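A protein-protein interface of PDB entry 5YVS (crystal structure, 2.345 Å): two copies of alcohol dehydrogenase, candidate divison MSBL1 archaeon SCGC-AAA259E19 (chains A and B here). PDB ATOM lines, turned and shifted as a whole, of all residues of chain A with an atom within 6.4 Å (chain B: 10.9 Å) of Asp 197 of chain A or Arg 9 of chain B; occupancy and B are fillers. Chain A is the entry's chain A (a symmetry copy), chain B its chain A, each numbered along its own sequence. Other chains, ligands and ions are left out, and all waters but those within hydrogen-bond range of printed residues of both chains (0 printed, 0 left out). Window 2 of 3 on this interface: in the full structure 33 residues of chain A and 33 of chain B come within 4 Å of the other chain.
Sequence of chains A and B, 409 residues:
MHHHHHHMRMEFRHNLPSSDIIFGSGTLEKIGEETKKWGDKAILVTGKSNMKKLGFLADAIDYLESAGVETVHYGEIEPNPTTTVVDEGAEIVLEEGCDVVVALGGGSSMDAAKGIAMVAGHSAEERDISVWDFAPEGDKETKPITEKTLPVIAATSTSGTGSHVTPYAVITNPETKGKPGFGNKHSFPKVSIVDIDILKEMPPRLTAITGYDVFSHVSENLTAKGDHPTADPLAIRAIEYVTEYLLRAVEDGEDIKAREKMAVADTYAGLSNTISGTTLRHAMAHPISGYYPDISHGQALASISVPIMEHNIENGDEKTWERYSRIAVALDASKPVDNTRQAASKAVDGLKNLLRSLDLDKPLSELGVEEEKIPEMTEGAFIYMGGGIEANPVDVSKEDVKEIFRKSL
The backbone NH of Met 10 of chain B sits at hydrogen-bond distance from the side-chain carboxylate of Glu 260 of chain A (3.0 Å). NE2 of His 7 of chain B lies within hydrogen-bond range of OE1 of Glu 260 of chain A, at 2.9 Å. OD1 of Asp 197 of chain A is in salt-bridge range of NH1 of Arg 9 of chain B, 3.5 Å away.
The backbone carbonyl oxygen of Gly 24 of chain A lies within hydrogen-bond range of the backbone NH of Ile 196 of chain A. OD2 of Asp 197 of chain A is in hydrogen-bond range of N of Gly 26 of chain A (3.3 Å). The side-chain carboxylate of Asp 195 of chain A is in hydrogen-bond range of the backbone NH of Asp 197 of chain A (2.9 Å). O of Gly 24 of chain A lies within hydrogen-bond range of OG1 of Thr 27 of chain A (3.3 Å). The backbone NH (N) of Thr 27 of chain A sits at hydrogen-bond distance from the side-chain carboxylate (OD2) of Asp 195 of chain A, at 3.2 Å.
Among the printed residues, merely in contact across the chains: Gly 24 of chain A with Met 10 of chain B (3.4 Å), Gly 24 of chain A with Glu 11 of chain B (3.8 Å), Ser 25 of chain A with Arg 9 of chain B (3.4 Å), Ser 25 of chain A with Glu 11 of chain B (3.97 Å), Thr 27 of chain A with Glu 11 of chain B (3.9 Å), Ile 196 of chain A with Arg 9 of chain B (3.9 Å), Ile 256 of chain A with Arg 9 of chain B (3.7 Å) and Glu 260 of chain A with Arg 9 of chain B (3.4 Å).
Of chain B, only Arg 9 comes within 4 Å of Asp 197 of chain A. Arg 9 of chain B touches just these residues of chain A: Ser 25, Ile 196, Asp 197, Ile 256 and Glu 260. No residue of chain B comes within 4 Å of Gly 26 of chain A. No residue of chain B comes within 4 Å of Asp 195 of chain A. Printed residues of chain B within 4 Å of Ile 196 of chain A: Arg 9. No residue of chain B comes within 4 Å of Ile 198 of chain A. Of the printed residues of chain B, Ile 256 of chain A touches Arg 9. Printed residues of chain B within 4 Å of Gly 24 of chain A: Met 10 and Glu 11. Of the printed residues of chain A, His 7 of chain B touches Glu 260 (2.9 Å). Of the printed residues of chain B, Glu 260 of chain A touches His 7, Arg 9 and Met 10. Printed residues of chain A within 4 Å of Glu 11 of chain B: Gly 24, Ser 25 and Thr 27. Printed residues of chain B within 4 Å of Thr 27 of chain A: Glu 11. Asp 227 of chain B touches none of the printed residues of chain A. The nearest residue of chain A that does not touch Arg 9 of chain B is Lys 200 of chain A (5.1 Å).
Of the 12 printed residues of chain B, 4 touch a printed residue of chain A. Printed residues of chain B that touch a printed residue of chain A: His 7, Arg 9, Met 10 and Glu 11. Hydrophobic or aromatic side chains of chain B within 4 Å of the printed part of chain A: His 7 and Met 10. Among the printed residues, 11 pairs touch across the chains. Among the printed residues, Asp or Glu carboxylates within 4 Å of a Lys or Arg side-chain nitrogen of the other chain: Asp 197 of chain A with Arg 9 of chain B.
No position is printed for both chains. Of the 11 pairs that touch across the chains among the printed residues, none has its exchanged pair printed and touching as well.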
ATOM      1  N   GLY A  24      -3.237  23.736   0.641  1.00  0.00           N
ATOM      2  CA  GLY A  24      -2.519  22.818  -0.221  1.00  0.00           C
ATOM      3  C   GLY A  24      -1.508  22.032   0.587  1.00  0.00           C
ATOM      4  O   GLY A  24      -1.445  22.126   1.810  1.00  0.00           O
ATOM      5  N   SER A  25      -0.711  21.248  -0.128  1.00  0.00           N
ATOM      6  CA  SER A  25       0.366  20.484   0.483  1.00  0.00           C
ATOM      7  C   SER A  25       1.685  21.177   0.179  1.00  0.00           C
ATOM      8  O   SER A  25       1.952  21.542  -0.971  1.00  0.00           O
ATOM      9  CB  SER A  25       0.376  19.036  -0.015  1.00  0.00           C
ATOM     10  OG  SER A  25       0.831  18.941  -1.353  1.00  0.00           O
ATOM     11  N   GLY A  26       2.499  21.367   1.213  1.00  0.00           N
ATOM     12  CA  GLY A  26       3.727  22.124   1.085  1.00  0.00           C
ATOM     13  C   GLY A  26       3.562  23.623   1.171  1.00  0.00           C
ATOM     14  O   GLY A  26       4.496  24.355   0.820  1.00  0.00           O
ATOM     15  N   THR A  27       2.401  24.106   1.618  1.00  0.00           N
ATOM     16  CA  THR A  27       2.163  25.533   1.771  1.00  0.00           C
ATOM     17  C   THR A  27       2.862  26.124   2.988  1.00  0.00           C
ATOM     18  O   THR A  27       2.840  27.347   3.161  1.00  0.00           O
ATOM     19  CB  THR A  27       0.663  25.809   1.854  1.00  0.00           C
ATOM     20  OG1 THR A  27       0.065  24.905   2.793  1.00  0.00           O
ATOM     21  CG2 THR A  27       0.018  25.624   0.489  1.00  0.00           C
ATOM     22  N   PHE A  56       8.844  19.721  10.741  1.00  0.00           N
ATOM     23  CA  PHE A  56       8.211  20.943  10.260  1.00  0.00           C
ATOM     24  C   PHE A  56       8.625  22.163  11.075  1.00  0.00           C
ATOM     25  O   PHE A  56       8.584  23.284  10.557  1.00  0.00           O
ATOM     26  CB  PHE A  56       6.688  20.787  10.267  1.00  0.00           C
ATOM     27  CG  PHE A  56       6.187  19.719   9.341  1.00  0.00           C
ATOM     28  CD1 PHE A  56       6.285  19.871   7.966  1.00  0.00           C
ATOM     29  CD2 PHE A  56       5.617  18.560   9.843  1.00  0.00           C
ATOM     30  CE1 PHE A  56       5.823  18.887   7.108  1.00  0.00           C
ATOM     31  CE2 PHE A  56       5.151  17.572   8.991  1.00  0.00           C
ATOM     32  CZ  PHE A  56       5.254  17.735   7.622  1.00  0.00           C
ATOM     33  N   ASP A 195      -1.619  23.010   5.493  1.00  0.00           N
ATOM     34  CA  ASP A 195      -0.661  22.196   4.750  1.00  0.00           C
ATOM     35  C   ASP A 195      -1.020  20.726   4.945  1.00  0.00           C
ATOM     36  O   ASP A 195      -0.929  20.203   6.060  1.00  0.00           O
ATOM     37  CB  ASP A 195       0.767  22.483   5.215  1.00  0.00           C
ATOM     38  CG  ASP A 195       1.817  21.871   4.305  1.00  0.00           C
ATOM     39  OD1 ASP A 195       1.516  20.857   3.638  1.00  0.00           O
ATOM     40  OD2 ASP A 195       2.948  22.404   4.261  1.00  0.00           O
ATOM     41  N   ILE A 196      -1.414  20.063   3.855  1.00  0.00           N
ATOM     42  CA  ILE A 196      -1.822  18.663   3.936  1.00  0.00           C
ATOM     43  C   ILE A 196      -0.670  17.771   4.382  1.00  0.00           C
ATOM     44  O   ILE A 196      -0.892  16.721   4.998  1.00  0.00           O
ATOM     45  CB  ILE A 196      -2.399  18.206   2.583  1.00  0.00           C
ATOM     46  CG1 ILE A 196      -3.622  19.048   2.215  1.00  0.00           C
ATOM     47  CG2 ILE A 196      -2.754  16.727   2.622  1.00  0.00           C
ATOM     48  CD1 ILE A 196      -4.724  19.006   3.247  1.00  0.00           C
ATOM     49  N   ASP A 197       0.573  18.158   4.080  1.00  0.00           N
ATOM     50  CA  ASP A 197       1.706  17.335   4.490  1.00  0.00           C
ATOM     51  C   ASP A 197       1.872  17.315   6.003  1.00  0.00           C
ATOM     52  O   ASP A 197       2.431  16.360   6.550  1.00  0.00           O
ATOM     53  CB  ASP A 197       2.989  17.830   3.830  1.00  0.00           C
ATOM     54  CG  ASP A 197       2.957  17.690   2.332  1.00  0.00           C
ATOM     55  OD1 ASP A 197       2.144  16.884   1.829  1.00  0.00           O
ATOM     56  OD2 ASP A 197       3.741  18.380   1.656  1.00  0.00           O
ATOM     57  N   ILE A 198       1.408  18.357   6.690  1.00  0.00           N
ATOM     58  CA  ILE A 198       1.457  18.354   8.147  1.00  0.00           C
ATOM     59  C   ILE A 198       0.273  17.590   8.718  1.00  0.00           C
ATOM     60  O   ILE A 198       0.422  16.802   9.658  1.00  0.00           O
ATOM     61  CB  ILE A 198       1.503  19.797   8.678  1.00  0.00           C
ATOM     62  CG1 ILE A 198       2.736  20.528   8.147  1.00  0.00           C
ATOM     63  CG2 ILE A 198       1.483  19.798  10.195  1.00  0.00           C
ATOM     64  CD1 ILE A 198       2.794  21.986   8.548  1.00  0.00           C
ATOM     65  N   LEU A 199      -0.916  17.806   8.153  1.00  0.00           N
ATOM     66  CA  LEU A 199      -2.125  17.191   8.693  1.00  0.00           C
ATOM     67  C   LEU A 199      -2.099  15.678   8.538  1.00  0.00           C
ATOM     68  O   LEU A 199      -2.498  14.952   9.454  1.00  0.00           O
ATOM     69  CB  LEU A 199      -3.358  17.772   8.005  1.00  0.00           C
ATOM     70  CG  LEU A 199      -3.526  19.285   8.091  1.00  0.00           C
ATOM     71  CD1 LEU A 199      -4.679  19.717   7.205  1.00  0.00           C
ATOM     72  CD2 LEU A 199      -3.757  19.715   9.530  1.00  0.00           C
ATOM     73  N   LYS A 200      -1.636  15.182   7.387  1.00  0.00           N
ATOM     74  CA  LYS A 200      -1.641  13.745   7.141  1.00  0.00           C
ATOM     75  C   LYS A 200      -0.823  12.967   8.162  1.00  0.00           C
ATOM     76  O   LYS A 200      -0.952  11.739   8.221  1.00  0.00           O
ATOM     77  CB  LYS A 200      -1.115  13.440   5.737  1.00  0.00           C
ATOM     78  CG  LYS A 200       0.383  13.628   5.588  1.00  0.00           C
ATOM     79  CD  LYS A 200       0.874  13.145   4.234  1.00  0.00           C
ATOM     80  CE  LYS A 200       2.376  13.320   4.116  1.00  0.00           C
ATOM     81  NZ  LYS A 200       2.983  12.324   3.196  1.00  0.00           N
ATOM     82  N   GLU A 201       0.011  13.635   8.956  1.00  0.00           N
ATOM     83  CA  GLU A 201       0.806  12.940   9.959  1.00  0.00           C
ATOM     84  C   GLU A 201       0.064  12.738  11.272  1.00  0.00           C
ATOM     85  O   GLU A 201       0.615  12.116  12.186  1.00  0.00           O
ATOM     86  CB  GLU A 201       2.114  13.692  10.216  1.00  0.00           C
ATOM     87  CG  GLU A 201       3.019  13.772   8.997  1.00  0.00           C
ATOM     88  CD  GLU A 201       3.504  12.408   8.533  1.00  0.00           C
ATOM     89  OE1 GLU A 201       3.645  11.502   9.383  1.00  0.00           O
ATOM     90  OE2 GLU A 201       3.743  12.243   7.317  1.00  0.00           O
ATOM     91  N   ILE A 256      -4.969  10.809   0.976  1.00  0.00           N
ATOM     92  CA  ILE A 256      -4.833  12.255   0.830  1.00  0.00           C
ATOM     93  C   ILE A 256      -6.186  12.909   0.573  1.00  0.00           C
ATOM     94  O   ILE A 256      -6.487  13.974   1.125  1.00  0.00           O
ATOM     95  CB  ILE A 256      -3.822  12.587  -0.284  1.00  0.00           C
ATOM     96  CG1 ILE A 256      -2.489  11.882  -0.021  1.00  0.00           C
ATOM     97  CG2 ILE A 256      -3.633  14.095  -0.399  1.00  0.00           C
ATOM     98  CD1 ILE A 256      -1.877  12.204   1.330  1.00  0.00           C
ATOM     99  N   GLU A 260      -7.713  15.921   2.690  1.00  0.00           N
ATOM    100  CA  GLU A 260      -8.116  17.194   2.101  1.00  0.00           C
ATOM    101  C   GLU A 260      -9.553  17.542   2.467  1.00  0.00           C
ATOM    102  O   GLU A 260      -9.861  18.700   2.767  1.00  0.00           O
ATOM    103  CB  GLU A 260      -7.951  17.150   0.584  1.00  0.00           C
ATOM    104  CG  GLU A 260      -6.516  17.040   0.122  1.00  0.00           C
ATOM    105  CD  GLU A 260      -6.416  16.856  -1.377  1.00  0.00           C
ATOM    106  OE1 GLU A 260      -7.447  16.547  -2.013  1.00  0.00           O
ATOM    107  OE2 GLU A 260      -5.309  17.023  -1.926  1.00  0.00           O
ATOM    108  N   HIS B   7      -3.912  10.435  -7.194  1.00  0.00           N
ATOM    109  CA  HIS B   7      -4.868  11.463  -6.798  1.00  0.00           C
ATOM    110  C   HIS B   7      -4.370  12.877  -7.124  1.00  0.00           C
ATOM    111  O   HIS B   7      -3.220  13.223  -6.847  1.00  0.00           O
ATOM    112  CB  HIS B   7      -5.179  11.350  -5.300  1.00  0.00           C
ATOM    113  CG  HIS B   7      -5.942  12.516  -4.747  1.00  0.00           C
ATOM    114  ND1 HIS B   7      -7.268  12.748  -5.043  1.00  0.00           N
ATOM    115  CD2 HIS B   7      -5.560  13.517  -3.917  1.00  0.00           C
ATOM    116  CE1 HIS B   7      -7.670  13.842  -4.419  1.00  0.00           C
ATOM    117  NE2 HIS B   7      -6.653  14.327  -3.730  1.00  0.00           N
ATOM    118  N   MET B   8      -5.250  13.682  -7.723  1.00  0.00           N
ATOM    119  CA  MET B   8      -4.969  15.093  -7.971  1.00  0.00           C
ATOM    120  C   MET B   8      -5.091  15.881  -6.671  1.00  0.00           C
ATOM    121  O   MET B   8      -6.157  15.899  -6.047  1.00  0.00           O
ATOM    122  CB  MET B   8      -5.934  15.654  -9.017  1.00  0.00           C
ATOM    123  CG  MET B   8      -5.831  15.040 -10.409  1.00  0.00           C
ATOM    124  SD  MET B   8      -6.935  15.826 -11.615  1.00  0.00           S
ATOM    125  CE  MET B   8      -6.730  17.565 -11.218  1.00  0.00           C
ATOM    126  N   ARG B   9      -4.009  16.542  -6.269  1.00  0.00           N
ATOM    127  CA  ARG B   9      -4.007  17.307  -5.032  1.00  0.00           C
ATOM    128  C   ARG B   9      -4.826  18.588  -5.178  1.00  0.00           C
ATOM    129  O   ARG B   9      -5.025  19.114  -6.277  1.00  0.00           O
ATOM    130  CB  ARG B   9      -2.580  17.657  -4.613  1.00  0.00           C
ATOM    131  CG  ARG B   9      -1.716  16.454  -4.301  1.00  0.00           C
ATOM    132  CD  ARG B   9      -1.503  16.294  -2.804  1.00  0.00           C
ATOM    133  NE  ARG B   9      -0.608  15.179  -2.504  1.00  0.00           N
ATOM    134  CZ  ARG B   9      -0.086  14.940  -1.307  1.00  0.00           C
ATOM    135  NH1 ARG B   9      -0.364  15.742  -0.289  1.00  0.00           N
ATOM    136  NH2 ARG B   9       0.720  13.901  -1.128  1.00  0.00           N
ATOM    137  N   MET B  10      -5.283  19.100  -4.038  1.00  0.00           N
ATOM    138  CA  MET B  10      -6.125  20.288  -3.986  1.00  0.00           C
ATOM    139  C   MET B  10      -5.292  21.495  -3.575  1.00  0.00           C
ATOM    140  O   MET B  10      -4.552  21.441  -2.587  1.00  0.00           O
ATOM    141  CB  MET B  10      -7.281  20.084  -3.008  1.00  0.00           C
ATOM    142  CG  MET B  10      -8.378  21.116  -3.115  1.00  0.00           C
ATOM    143  SD  MET B  10      -9.546  20.976  -1.752  1.00  0.00           S
ATOM    144  CE  MET B  10     -10.134  19.302  -1.975  1.00  0.00           C
ATOM    145  N   GLU B  11      -5.416  22.580  -4.335  1.00  0.00           N
ATOM    146  CA  GLU B  11      -4.665  23.801  -4.082  1.00  0.00           C
ATOM    147  C   GLU B  11      -5.558  25.001  -4.351  1.00  0.00           C
ATOM    148  O   GLU B  11      -6.206  25.070  -5.399  1.00  0.00           O
ATOM    149  CB  GLU B  11      -3.414  23.870  -4.963  1.00  0.00           C
ATOM    150  CG  GLU B  11      -2.173  23.266  -4.334  1.00  0.00           C
ATOM    151  CD  GLU B  11      -1.156  24.323  -3.948  1.00  0.00           C
ATOM    152  OE1 GLU B  11      -0.314  24.048  -3.065  1.00  0.00           O
ATOM    153  OE2 GLU B  11      -1.202  25.431  -4.529  1.00  0.00           O
ATOM    154  N   PHE B  12      -5.588  25.941  -3.409  1.00  0.00           N
ATOM    155  CA  PHE B  12      -6.350  27.166  -3.600  1.00  0.00           C
ATOM    156  C   PHE B  12      -5.959  28.167  -2.525  1.00  0.00           C
ATOM    157  O   PHE B  12      -5.430  27.805  -1.472  1.00  0.00           O
ATOM    158  CB  PHE B  12      -7.862  26.907  -3.570  1.00  0.00           C
ATOM    159  CG  PHE B  12      -8.386  26.489  -2.222  1.00  0.00           C
ATOM    160  CD1 PHE B  12      -8.500  25.148  -1.893  1.00  0.00           C
ATOM    161  CD2 PHE B  12      -8.779  27.437  -1.288  1.00  0.00           C
ATOM    162  CE1 PHE B  12      -8.988  24.762  -0.660  1.00  0.00           C
ATOM    163  CE2 PHE B  12      -9.266  27.056  -0.050  1.00  0.00           C
ATOM    164  CZ  PHE B  12      -9.370  25.716   0.264  1.00  0.00           C
ATOM    165  N   GLY B 226     -10.183  25.665 -11.441  1.00  0.00           N
ATOM    166  CA  GLY B 226      -9.480  25.476 -10.190  1.00  0.00           C
ATOM    167  C   GLY B 226     -10.404  25.083  -9.054  1.00  0.00           C
ATOM    168  O   GLY B 226     -11.614  24.914  -9.210  1.00  0.00           O
ATOM    169  N   ASP B 227      -9.804  24.935  -7.876  1.00  0.00           N
ATOM    170  CA  ASP B 227     -10.538  24.581  -6.671  1.00  0.00           C
ATOM    171  C   ASP B 227     -10.944  25.839  -5.913  1.00  0.00           C
ATOM    172  O   ASP B 227     -10.159  26.783  -5.789  1.00  0.00           O
ATOM    173  CB  ASP B 227      -9.692  23.678  -5.774  1.00  0.00           C
ATOM    174  CG  ASP B 227      -9.384  22.341  -6.419  1.00  0.00           C
ATOM    175  OD1 ASP B 227     -10.300  21.745  -7.021  1.00  0.00           O
ATOM    176  OD2 ASP B 227      -8.223  21.888  -6.329  1.00  0.00           O
ATOM    177  N   HIS B 228     -12.180  25.847  -5.414  1.00  0.00           N
ATOM    178  CA  HIS B 228     -12.697  26.951  -4.611  1.00  0.00           C
ATOM    179  C   HIS B 228     -13.773  26.435  -3.663  1.00  0.00           C
ATOM    180  O   HIS B 228     -14.928  26.873  -3.734  1.00  0.00           O
ATOM    181  CB  HIS B 228     -13.253  28.061  -5.504  1.00  0.00           C
ATOM    182  CG  HIS B 228     -13.814  27.573  -6.803  1.00  0.00           C
ATOM    183  ND1 HIS B 228     -14.971  26.827  -6.885  1.00  0.00           N
ATOM    184  CD2 HIS B 228     -13.375  27.728  -8.075  1.00  0.00           C
ATOM    185  CE1 HIS B 228     -15.220  26.543  -8.152  1.00  0.00           C
ATOM    186  NE2 HIS B 228     -14.267  27.079  -8.893  1.00  0.00           N
ATOM    187  N   PRO B 229     -13.429  25.517  -2.754  1.00  0.00           N
ATOM    188  CA  PRO B 229     -14.467  24.844  -1.956  1.00  0.00           C
ATOM    189  C   PRO B 229     -15.137  25.733  -0.923  1.00  0.00           C
ATOM    190  O   PRO B 229     -16.211  25.366  -0.430  1.00  0.00           O
ATOM    191  CB  PRO B 229     -13.706  23.694  -1.285  1.00  0.00           C
ATOM    192  CG  PRO B 229     -12.291  24.151  -1.241  1.00  0.00           C
ATOM    193  CD  PRO B 229     -12.078  25.013  -2.454  1.00  0.00           C
ATOM    194  N   LYS B 319     -14.274  16.593 -14.319  1.00  0.00           N
ATOM    195  CA  LYS B 319     -14.403  17.480 -13.166  1.00  0.00           C
ATOM    196  C   LYS B 319     -15.379  18.614 -13.446  1.00  0.00           C
ATOM    197  O   LYS B 319     -16.206  18.958 -12.593  1.00  0.00           O
ATOM    198  CB  LYS B 319     -13.037  18.041 -12.780  1.00  0.00           C
ATOM    199  CG  LYS B 319     -13.091  19.015 -11.623  1.00  0.00           C
ATOM    200  CD  LYS B 319     -11.738  19.642 -11.373  1.00  0.00           C
ATOM    201  CE  LYS B 319     -11.794  20.611 -10.212  1.00  0.00           C
ATOM    202  NZ  LYS B 319     -10.482  21.271  -9.993  1.00  0.00           N
ATOM    203  N   ARG B 323     -19.492  19.303 -11.942  1.00  0.00           N
ATOM    204  CA  ARG B 323     -20.010  20.560 -11.411  1.00  0.00           C
ATOM    205  C   ARG B 323     -21.312  20.954 -12.096  1.00  0.00           C
ATOM    206  O   ARG B 323     -22.279  21.342 -11.430  1.00  0.00           O
ATOM    207  CB  ARG B 323     -18.963  21.664 -11.560  1.00  0.00           C
ATOM    208  CG  ARG B 323     -17.818  21.558 -10.574  1.00  0.00           C
ATOM    209  CD  ARG B 323     -16.653  22.434 -10.989  1.00  0.00           C
ATOM    210  NE  ARG B 323     -15.679  22.589  -9.912  1.00  0.00           N
ATOM    211  CZ  ARG B 323     -14.552  23.283 -10.019  1.00  0.00           C
ATOM    212  NH1 ARG B 323     -14.248  23.887 -11.159  1.00  0.00           N
ATOM    213  NH2 ARG B 323     -13.724  23.373  -8.987  1.00  0.00           N
